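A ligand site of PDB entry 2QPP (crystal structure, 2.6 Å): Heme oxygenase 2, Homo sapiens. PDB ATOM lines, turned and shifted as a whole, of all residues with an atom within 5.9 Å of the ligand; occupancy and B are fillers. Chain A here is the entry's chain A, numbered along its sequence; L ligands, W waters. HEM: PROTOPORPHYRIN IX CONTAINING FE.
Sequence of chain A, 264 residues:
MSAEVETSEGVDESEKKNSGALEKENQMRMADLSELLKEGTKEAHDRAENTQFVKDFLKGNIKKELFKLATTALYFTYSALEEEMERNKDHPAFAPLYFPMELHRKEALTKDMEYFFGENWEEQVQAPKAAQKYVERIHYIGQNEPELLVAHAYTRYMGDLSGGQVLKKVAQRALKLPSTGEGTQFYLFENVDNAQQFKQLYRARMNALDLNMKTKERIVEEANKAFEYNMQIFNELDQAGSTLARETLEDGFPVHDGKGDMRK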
ATOM      1  N   SER A  34      -1.692   8.095   7.986  1.00  0.00           N
ATOM      2  CA  SER A  34      -1.976   9.015   6.886  1.00  0.00           C
ATOM      3  C   SER A  34      -0.922  10.107   6.731  1.00  0.00           C
ATOM      4  O   SER A  34      -0.608  10.513   5.614  1.00  0.00           O
ATOM      5  CB  SER A  34      -3.362   9.650   7.067  1.00  0.00           C
ATOM      6  OG  SER A  34      -3.371  10.601   8.116  1.00  0.00           O
ATOM      7  N   LEU A  37       2.359   8.273   5.506  1.00  0.00           N
ATOM      8  CA  LEU A  37       2.276   7.988   4.079  1.00  0.00           C
ATOM      9  C   LEU A  37       2.484   9.230   3.209  1.00  0.00           C
ATOM     10  O   LEU A  37       3.145   9.153   2.177  1.00  0.00           O
ATOM     11  CB  LEU A  37       0.940   7.325   3.747  1.00  0.00           C
ATOM     12  CG  LEU A  37       0.827   5.849   4.113  1.00  0.00           C
ATOM     13  CD1 LEU A  37      -0.618   5.424   4.113  1.00  0.00           C
ATOM     14  CD2 LEU A  37       1.617   4.971   3.153  1.00  0.00           C
ATOM     15  N   LYS A  38       1.939  10.362   3.643  1.00  0.00           N
ATOM     16  CA  LYS A  38       2.058  11.594   2.873  1.00  0.00           C
ATOM     17  C   LYS A  38       3.479  12.159   2.913  1.00  0.00           C
ATOM     18  O   LYS A  38       4.030  12.536   1.882  1.00  0.00           O
ATOM     19  CB  LYS A  38       1.041  12.647   3.338  1.00  0.00           C
ATOM     20  CG  LYS A  38       0.768  13.704   2.291  1.00  0.00           C
ATOM     21  CD  LYS A  38       0.098  14.933   2.878  1.00  0.00           C
ATOM     22  CE  LYS A  38      -0.272  15.924   1.775  1.00  0.00           C
ATOM     23  NZ  LYS A  38      -1.043  17.094   2.303  1.00  0.00           N
ATOM     24  N   THR A  41       5.957   9.463   1.191  1.00  0.00           N
ATOM     25  CA  THR A  41       5.906   9.279  -0.272  1.00  0.00           C
ATOM     26  C   THR A  41       5.982  10.606  -1.055  1.00  0.00           C
ATOM     27  O   THR A  41       5.672  10.640  -2.250  1.00  0.00           O
ATOM     28  CB  THR A  41       4.640   8.500  -0.729  1.00  0.00           C
ATOM     29  OG1 THR A  41       3.474   9.215  -0.349  1.00  0.00           O
ATOM     30  CG2 THR A  41       4.610   7.094  -0.121  1.00  0.00           C
ATOM     31  N   HIS A  45       5.861  11.197  -5.100  1.00  0.00           N
ATOM     32  CA  HIS A  45       4.762  11.949  -5.710  1.00  0.00           C
ATOM     33  C   HIS A  45       5.287  13.058  -6.627  1.00  0.00           C
ATOM     34  O   HIS A  45       4.747  13.273  -7.724  1.00  0.00           O
ATOM     35  CB  HIS A  45       3.822  12.518  -4.655  1.00  0.00           C
ATOM     36  CG  HIS A  45       2.490  12.926  -5.196  1.00  0.00           C
ATOM     37  ND1 HIS A  45       2.242  14.201  -5.675  1.00  0.00           N
ATOM     38  CD2 HIS A  45       1.337  12.243  -5.333  1.00  0.00           C
ATOM     39  CE1 HIS A  45       0.987  14.275  -6.092  1.00  0.00           C
ATOM     40  NE2 HIS A  45       0.415  13.103  -5.890  1.00  0.00           N
ATOM     41  N   ALA A  48       6.280  11.354  -9.792  1.00  0.00           N
ATOM     42  CA  ALA A  48       5.076  11.038 -10.563  1.00  0.00           C
ATOM     43  C   ALA A  48       4.463  12.270 -11.241  1.00  0.00           C
ATOM     44  O   ALA A  48       4.033  12.193 -12.397  1.00  0.00           O
ATOM     45  CB  ALA A  48       4.053  10.353  -9.676  1.00  0.00           C
ATOM     46  N   GLU A  49       4.430  13.400 -10.532  1.00  0.00           N
ATOM     47  CA  GLU A  49       3.925  14.658 -11.077  1.00  0.00           C
ATOM     48  C   GLU A  49       4.703  15.130 -12.316  1.00  0.00           C
ATOM     49  O   GLU A  49       4.120  15.734 -13.214  1.00  0.00           O
ATOM     50  CB  GLU A  49       3.962  15.779 -10.032  1.00  0.00           C
ATOM     51  CG  GLU A  49       2.815  15.783  -9.042  1.00  0.00           C
ATOM     52  CD  GLU A  49       2.767  17.049  -8.186  1.00  0.00           C
ATOM     53  OE1 GLU A  49       3.693  17.884  -8.278  1.00  0.00           O
ATOM     54  OE2 GLU A  49       1.811  17.210  -7.417  1.00  0.00           O
ATOM     55  N   ASN A  50       6.001  14.853 -12.347  1.00  0.00           N
ATOM     56  CA  ASN A  50       6.891  15.430 -13.343  1.00  0.00           C
ATOM     57  C   ASN A  50       7.426  14.461 -14.401  1.00  0.00           C
ATOM     58  O   ASN A  50       8.319  14.806 -15.172  1.00  0.00           O
ATOM     59  CB  ASN A  50       8.048  16.161 -12.655  1.00  0.00           C
ATOM     60  CG  ASN A  50       7.572  17.366 -11.864  1.00  0.00           C
ATOM     61  OD1 ASN A  50       7.143  18.379 -12.441  1.00  0.00           O
ATOM     62  ND2 ASN A  50       7.625  17.269 -10.540  1.00  0.00           N
ATOM     63  N   VAL A  54       2.977  11.695 -17.893  1.00  0.00           N
ATOM     64  CA  VAL A  54       1.974  12.454 -17.146  1.00  0.00           C
ATOM     65  C   VAL A  54       1.880  13.897 -17.650  1.00  0.00           C
ATOM     66  O   VAL A  54       0.772  14.412 -17.819  1.00  0.00           O
ATOM     67  CB  VAL A  54       2.239  12.394 -15.605  1.00  0.00           C
ATOM     68  CG1 VAL A  54       1.398  13.430 -14.862  1.00  0.00           C
ATOM     69  CG2 VAL A  54       1.929  11.015 -15.075  1.00  0.00           C
ATOM     70  N   LEU A  58      -1.429  15.610 -19.611  1.00  0.00           N
ATOM     71  CA  LEU A  58      -2.059  16.841 -19.146  1.00  0.00           C
ATOM     72  C   LEU A  58      -2.095  17.944 -20.197  1.00  0.00           C
ATOM     73  O   LEU A  58      -3.063  18.705 -20.269  1.00  0.00           O
ATOM     74  CB  LEU A  58      -1.409  17.316 -17.843  1.00  0.00           C
ATOM     75  CG  LEU A  58      -1.659  16.395 -16.647  1.00  0.00           C
ATOM     76  CD1 LEU A  58      -0.662  16.648 -15.550  1.00  0.00           C
ATOM     77  CD2 LEU A  58      -3.090  16.547 -16.112  1.00  0.00           C
ATOM     78  N   TYR A 154      -4.330   2.915  -0.924  1.00  0.00           N
ATOM     79  CA  TYR A 154      -3.937   4.302  -0.688  1.00  0.00           C
ATOM     80  C   TYR A 154      -3.391   4.963  -1.955  1.00  0.00           C
ATOM     81  O   TYR A 154      -3.932   5.973  -2.399  1.00  0.00           O
ATOM     82  CB  TYR A 154      -2.919   4.408   0.455  1.00  0.00           C
ATOM     83  CG  TYR A 154      -2.219   5.761   0.542  1.00  0.00           C
ATOM     84  CD1 TYR A 154      -2.815   6.841   1.199  1.00  0.00           C
ATOM     85  CD2 TYR A 154      -0.968   5.945  -0.055  1.00  0.00           C
ATOM     86  CE1 TYR A 154      -2.166   8.084   1.272  1.00  0.00           C
ATOM     87  CE2 TYR A 154      -0.321   7.182   0.007  1.00  0.00           C
ATOM     88  CZ  TYR A 154      -0.918   8.240   0.668  1.00  0.00           C
ATOM     89  OH  TYR A 154      -0.253   9.456   0.721  1.00  0.00           O
ATOM     90  N   THR A 155      -2.343   4.382  -2.523  1.00  0.00           N
ATOM     91  CA  THR A 155      -1.644   4.959  -3.677  1.00  0.00           C
ATOM     92  C   THR A 155      -2.569   5.173  -4.871  1.00  0.00           C
ATOM     93  O   THR A 155      -2.532   6.222  -5.512  1.00  0.00           O
ATOM     94  CB  THR A 155      -0.439   4.091  -4.086  1.00  0.00           C
ATOM     95  OG1 THR A 155       0.419   3.891  -2.954  1.00  0.00           O
ATOM     96  CG2 THR A 155       0.367   4.762  -5.185  1.00  0.00           C
ATOM     97  N   ARG A 156      -3.415   4.198  -5.153  1.00  0.00           N
ATOM     98  CA  ARG A 156      -4.295   4.287  -6.301  1.00  0.00           C
ATOM     99  C   ARG A 156      -5.547   5.147  -6.085  1.00  0.00           C
ATOM    100  O   ARG A 156      -5.735   6.147  -6.788  1.00  0.00           O
ATOM    101  CB  ARG A 156      -4.602   2.905  -6.862  1.00  0.00           C
ATOM    102  CG  ARG A 156      -3.547   2.479  -7.890  1.00  0.00           C
ATOM    103  CD  ARG A 156      -3.944   3.028  -9.242  1.00  0.00           C
ATOM    104  NE  ARG A 156      -2.900   3.757  -9.936  1.00  0.00           N
ATOM    105  CZ  ARG A 156      -3.128   4.777 -10.758  1.00  0.00           C
ATOM    106  NH1 ARG A 156      -4.375   5.209 -10.958  1.00  0.00           N
ATOM    107  NH2 ARG A 156      -2.110   5.387 -11.359  1.00  0.00           N
ATOM    108  N   MET A 158      -6.685   7.187  -3.516  1.00  0.00           N
ATOM    109  CA  MET A 158      -6.488   8.558  -3.031  1.00  0.00           C
ATOM    110  C   MET A 158      -6.040   9.500  -4.154  1.00  0.00           C
ATOM    111  O   MET A 158      -6.501  10.638  -4.233  1.00  0.00           O
ATOM    112  CB  MET A 158      -5.493   8.589  -1.876  1.00  0.00           C
ATOM    113  CG  MET A 158      -5.961   7.911  -0.586  1.00  0.00           C
ATOM    114  SD  MET A 158      -7.177   8.875   0.341  1.00  0.00           S
ATOM    115  CE  MET A 158      -8.695   8.150  -0.281  1.00  0.00           C
ATOM    116  N   GLY A 159      -5.139   9.016  -5.005  1.00  0.00           N
ATOM    117  CA  GLY A 159      -4.761   9.743  -6.219  1.00  0.00           C
ATOM    118  C   GLY A 159      -5.962   9.980  -7.117  1.00  0.00           C
ATOM    119  O   GLY A 159      -6.214  11.109  -7.530  1.00  0.00           O
ATOM    120  N   ASP A 160      -6.722   8.912  -7.392  1.00  0.00           N
ATOM    121  CA  ASP A 160      -7.920   8.971  -8.224  1.00  0.00           C
ATOM    122  C   ASP A 160      -8.933  10.016  -7.755  1.00  0.00           C
ATOM    123  O   ASP A 160      -9.543  10.694  -8.576  1.00  0.00           O
ATOM    124  CB  ASP A 160      -8.628   7.612  -8.266  1.00  0.00           C
ATOM    125  CG  ASP A 160      -7.807   6.538  -8.927  1.00  0.00           C
ATOM    126  OD1 ASP A 160      -6.931   6.882  -9.760  1.00  0.00           O
ATOM    127  OD2 ASP A 160      -8.031   5.348  -8.613  1.00  0.00           O
ATOM    128  N   SER A 162      -8.297  12.725  -6.135  1.00  0.00           N
ATOM    129  CA  SER A 162      -7.715  14.063  -6.104  1.00  0.00           C
ATOM    130  C   SER A 162      -7.675  14.739  -7.483  1.00  0.00           C
ATOM    131  O   SER A 162      -7.866  15.950  -7.586  1.00  0.00           O
ATOM    132  CB  SER A 162      -6.299  14.014  -5.504  1.00  0.00           C
ATOM    133  OG  SER A 162      -6.303  13.350  -4.250  1.00  0.00           O
ATOM    134  N   GLY A 163      -7.442  13.949  -8.532  1.00  0.00           N
ATOM    135  CA  GLY A 163      -7.228  14.505  -9.863  1.00  0.00           C
ATOM    136  C   GLY A 163      -8.164  14.035 -10.972  1.00  0.00           C
ATOM    137  O   GLY A 163      -8.066  14.521 -12.109  1.00  0.00           O
ATOM    138  N   GLN A 196     -13.310  15.267  -1.363  1.00  0.00           N
ATOM    139  CA  GLN A 196     -12.522  15.842  -0.282  1.00  0.00           C
ATOM    140  C   GLN A 196     -12.892  15.252   1.083  1.00  0.00           C
ATOM    141  O   GLN A 196     -12.014  14.855   1.847  1.00  0.00           O
ATOM    142  CB  GLN A 196     -12.642  17.371  -0.277  1.00  0.00           C
ATOM    143  CG  GLN A 196     -11.428  18.107   0.301  1.00  0.00           C
ATOM    144  CD  GLN A 196     -10.283  18.289  -0.717  1.00  0.00           C
ATOM    145  OE1 GLN A 196     -10.060  17.458  -1.603  1.00  0.00           O
ATOM    146  NE2 GLN A 196      -9.551  19.396  -0.581  1.00  0.00           N
ATOM    147  N   LYS A 199     -12.025  11.388   1.236  1.00  0.00           N
ATOM    148  CA  LYS A 199     -10.600  11.248   1.526  1.00  0.00           C
ATOM    149  C   LYS A 199     -10.292  11.405   3.014  1.00  0.00           C
ATOM    150  O   LYS A 199      -9.445  10.693   3.549  1.00  0.00           O
ATOM    151  CB  LYS A 199      -9.787  12.262   0.708  1.00  0.00           C
ATOM    152  CG  LYS A 199      -9.494  11.840  -0.723  1.00  0.00           C
ATOM    153  CD  LYS A 199      -8.444  12.751  -1.364  1.00  0.00           C
ATOM    154  CE  LYS A 199      -8.987  14.138  -1.666  1.00  0.00           C
ATOM    155  NZ  LYS A 199      -7.903  15.096  -2.045  1.00  0.00           N
ATOM    156  N   ARG A 203      -8.697   8.600   5.497  1.00  0.00           N
ATOM    157  CA  ARG A 203      -7.547   8.903   6.356  1.00  0.00           C
ATOM    158  C   ARG A 203      -7.841   8.526   7.804  1.00  0.00           C
ATOM    159  O   ARG A 203      -6.993   7.946   8.487  1.00  0.00           O
ATOM    160  CB  ARG A 203      -7.175  10.379   6.285  1.00  0.00           C
ATOM    161  CG  ARG A 203      -6.479  10.795   5.000  1.00  0.00           C
ATOM    162  CD  ARG A 203      -6.007  12.233   5.082  1.00  0.00           C
ATOM    163  NE  ARG A 203      -5.501  12.699   3.789  1.00  0.00           N
ATOM    164  CZ  ARG A 203      -6.198  13.426   2.922  1.00  0.00           C
ATOM    165  NH1 ARG A 203      -7.445  13.790   3.208  1.00  0.00           N
ATOM    166  NH2 ARG A 203      -5.654  13.792   1.777  1.00  0.00           N
ATOM    167  N   PHE A 227       4.048   3.432  -6.096  1.00  0.00           N
ATOM    168  CA  PHE A 227       4.335   4.576  -6.965  1.00  0.00           C
ATOM    169  C   PHE A 227       5.281   4.198  -8.093  1.00  0.00           C
ATOM    170  O   PHE A 227       5.106   4.620  -9.236  1.00  0.00           O
ATOM    171  CB  PHE A 227       4.954   5.729  -6.161  1.00  0.00           C
ATOM    172  CG  PHE A 227       3.934   6.679  -5.565  1.00  0.00           C
ATOM    173  CD1 PHE A 227       3.511   6.527  -4.254  1.00  0.00           C
ATOM    174  CD2 PHE A 227       3.423   7.748  -6.323  1.00  0.00           C
ATOM    175  CE1 PHE A 227       2.587   7.411  -3.701  1.00  0.00           C
ATOM    176  CE2 PHE A 227       2.504   8.630  -5.778  1.00  0.00           C
ATOM    177  CZ  PHE A 227       2.081   8.456  -4.463  1.00  0.00           C
ATOM    178  N   ASN A 230       3.762   2.296 -10.915  1.00  0.00           N
ATOM    179  CA  ASN A 230       3.153   3.292 -11.789  1.00  0.00           C
ATOM    180  C   ASN A 230       4.180   4.012 -12.655  1.00  0.00           C
ATOM    181  O   ASN A 230       3.935   4.241 -13.845  1.00  0.00           O
ATOM    182  CB  ASN A 230       2.295   4.295 -11.002  1.00  0.00           C
ATOM    183  CG  ASN A 230       1.043   3.668 -10.414  1.00  0.00           C
ATOM    184  OD1 ASN A 230      -0.026   3.708 -11.027  1.00  0.00           O
ATOM    185  ND2 ASN A 230       1.178   3.059  -9.235  1.00  0.00           N
ATOM    186  N   PHE A 234       4.106   4.219 -16.699  1.00  0.00           N
ATOM    187  CA  PHE A 234       4.257   5.529 -17.338  1.00  0.00           C
ATOM    188  C   PHE A 234       5.451   5.541 -18.287  1.00  0.00           C
ATOM    189  O   PHE A 234       5.362   6.069 -19.403  1.00  0.00           O
ATOM    190  CB  PHE A 234       4.443   6.642 -16.310  1.00  0.00           C
ATOM    191  CG  PHE A 234       3.229   6.933 -15.477  1.00  0.00           C
ATOM    192  CD1 PHE A 234       1.945   6.669 -15.955  1.00  0.00           C
ATOM    193  CD2 PHE A 234       3.372   7.503 -14.216  1.00  0.00           C
ATOM    194  CE1 PHE A 234       0.827   6.953 -15.189  1.00  0.00           C
ATOM    195  CE2 PHE A 234       2.256   7.794 -13.438  1.00  0.00           C
ATOM    196  CZ  PHE A 234       0.981   7.520 -13.921  1.00  0.00           C
HETATM  197  CHA HEM L   1      -2.938  13.557  -3.633  1.00  0.00           C
HETATM  198  CHB HEM L   1      -1.983  16.244  -7.519  1.00  0.00           C
HETATM  199  CHC HEM L   1      -0.407  12.341  -9.949  1.00  0.00           C
HETATM  200  CHD HEM L   1      -1.067   9.659  -5.930  1.00  0.00           C
HETATM  201  C1A HEM L   1      -2.750  14.657  -4.438  1.00  0.00           C
HETATM  202  C2A HEM L   1      -2.905  16.055  -4.071  1.00  0.00           C
HETATM  203  C3A HEM L   1      -2.637  16.785  -5.164  1.00  0.00           C
HETATM  204  C4A HEM L   1      -2.312  15.879  -6.235  1.00  0.00           C
HETATM  205  CMA HEM L   1      -2.663  18.338  -5.259  1.00  0.00           C
HETATM  206  CAA HEM L   1      -3.289  16.630  -2.686  1.00  0.00           C
HETATM  207  CBA HEM L   1      -4.712  16.247  -2.256  1.00  0.00           C
HETATM  208  CGA HEM L   1      -4.886  16.425  -0.765  1.00  0.00           C
HETATM  209  O1A HEM L   1      -6.025  16.777  -0.327  1.00  0.00           O
HETATM  210  O2A HEM L   1      -3.897  16.216   0.001  1.00  0.00           O
HETATM  211  C1B HEM L   1      -1.436  15.440  -8.492  1.00  0.00           C
HETATM  212  C2B HEM L   1      -0.919  15.903  -9.752  1.00  0.00           C
HETATM  213  C3B HEM L   1      -0.485  14.828 -10.437  1.00  0.00           C
HETATM  214  C4B HEM L   1      -0.703  13.649  -9.624  1.00  0.00           C
HETATM  215  CMB HEM L   1      -0.900  17.385 -10.198  1.00  0.00           C
HETATM  216  CAB HEM L   1       0.157  14.841 -11.850  1.00  0.00           C
HETATM  217  CBB HEM L   1       0.450  16.004 -12.445  1.00  0.00           C
HETATM  218  C1C HEM L   1      -0.430  11.271  -9.071  1.00  0.00           C
HETATM  219  C2C HEM L   1       0.015   9.918  -9.343  1.00  0.00           C
HETATM  220  C3C HEM L   1      -0.165   9.183  -8.235  1.00  0.00           C
HETATM  221  C4C HEM L   1      -0.733  10.038  -7.214  1.00  0.00           C
HETATM  222  CMC HEM L   1       0.603   9.443 -10.691  1.00  0.00           C
HETATM  223  CAC HEM L   1       0.168   7.691  -8.048  1.00  0.00           C
HETATM  224  CBC HEM L   1      -0.469   6.743  -8.734  1.00  0.00           C
HETATM  225  C1D HEM L   1      -1.610  10.440  -4.937  1.00  0.00           C
HETATM  226  C2D HEM L   1      -1.910   9.999  -3.591  1.00  0.00           C
HETATM  227  C3D HEM L   1      -2.489  11.213  -2.888  1.00  0.00           C
HETATM  228  C4D HEM L   1      -2.492  12.269  -3.869  1.00  0.00           C
HETATM  229  CMD HEM L   1      -1.702   8.601  -2.965  1.00  0.00           C
HETATM  230  CAD HEM L   1      -2.985  11.305  -1.432  1.00  0.00           C
HETATM  231  CBD HEM L   1      -2.006  12.118  -0.601  1.00  0.00           C
HETATM  232  CGD HEM L   1      -2.548  12.113   0.793  1.00  0.00           C
HETATM  233  O1D HEM L   1      -3.491  12.901   1.068  1.00  0.00           O
HETATM  234  O2D HEM L   1      -2.049  11.306   1.612  1.00  0.00           O
HETATM  235  NA  HEM L   1      -2.390  14.584  -5.771  1.00  0.00           N
HETATM  236  NB  HEM L   1      -1.290  14.057  -8.436  1.00  0.00           N
HETATM  237  NC  HEM L   1      -0.878  11.312  -7.756  1.00  0.00           N
HETATM  238  ND  HEM L   1      -1.967  11.776  -5.059  1.00  0.00           N
HETATM  239 FE   HEM L   1      -1.479  12.937  -6.683  1.00  0.00          FE
HETATM  240  O   HOH W   1      -3.433  12.379  -8.007  1.00  0.00           O
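FE of the ligand is bound by NE2 of His 45, at 2.1 Å.
NH2 of Arg 203 lies within salt-bridge range of O1D of the ligand (2.4 Å).
O2D of the ligand is in hydrogen-bond range of OH of Tyr 154, 2.7 Å away.
An oxygen (O1A) of the ligand is in salt-bridge range of the side-chain amino group (NZ) of Lys 199.
The side-chain amino group (NZ) of Lys 38 is in salt-bridge range of an oxygen (O2A) of the ligand (3.8 Å).
Merely in contact with the ligand: Ala 48 (3.7 Å), Glu 49 (3.7 Å), Val 54 (3.6 Å), Leu 58 (3.4 Å), Thr 155 (3.6 Å), Arg 156 (3.4 Å), Met 158 (3.7 Å), Gly 159 (3.5 Å), Ser 162 (3.4 Å), Phe 227 (3.4 Å), Asn 230 (3.8 Å) and Phe 234 (3.6 Å).
Hydrophobic or aromatic side chains within 4 Å of the ligand: His 45, Ala 48, Val 54, Leu 58, Tyr 154, Met 158, Phe 227 and Phe 234.
Of the 24 residues printed, 17 come within 4 Å of the ligand.
Along chain A the residues within 4 Å of the ligand span positions 38 to 234.
The nearest printed residue that does not touch the ligand is Gln 196 (4.3 Å).
The side-chain amino group of Lys 199 sits at hydrogen-bond distance from the side-chain hydroxyl of Ser 162 (3.2 Å).
NZ of Lys 199 sits at hydrogen-bond distance from OE1 of Gln 196 (3.2 Å).
NH2 of Arg 156 is in hydrogen-bond range of OD1 of Asn 230 (2.7 Å).
The guanidinium group (NH1) of Arg 156 lies within salt-bridge range of the side-chain carboxylate (OD1) of Asp 160, at 3.3 Å.
The side-chain hydroxyl (OG) of Ser 162 is in hydrogen-bond range of the backbone carbonyl oxygen (O) of Met 158 (2.7 Å).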
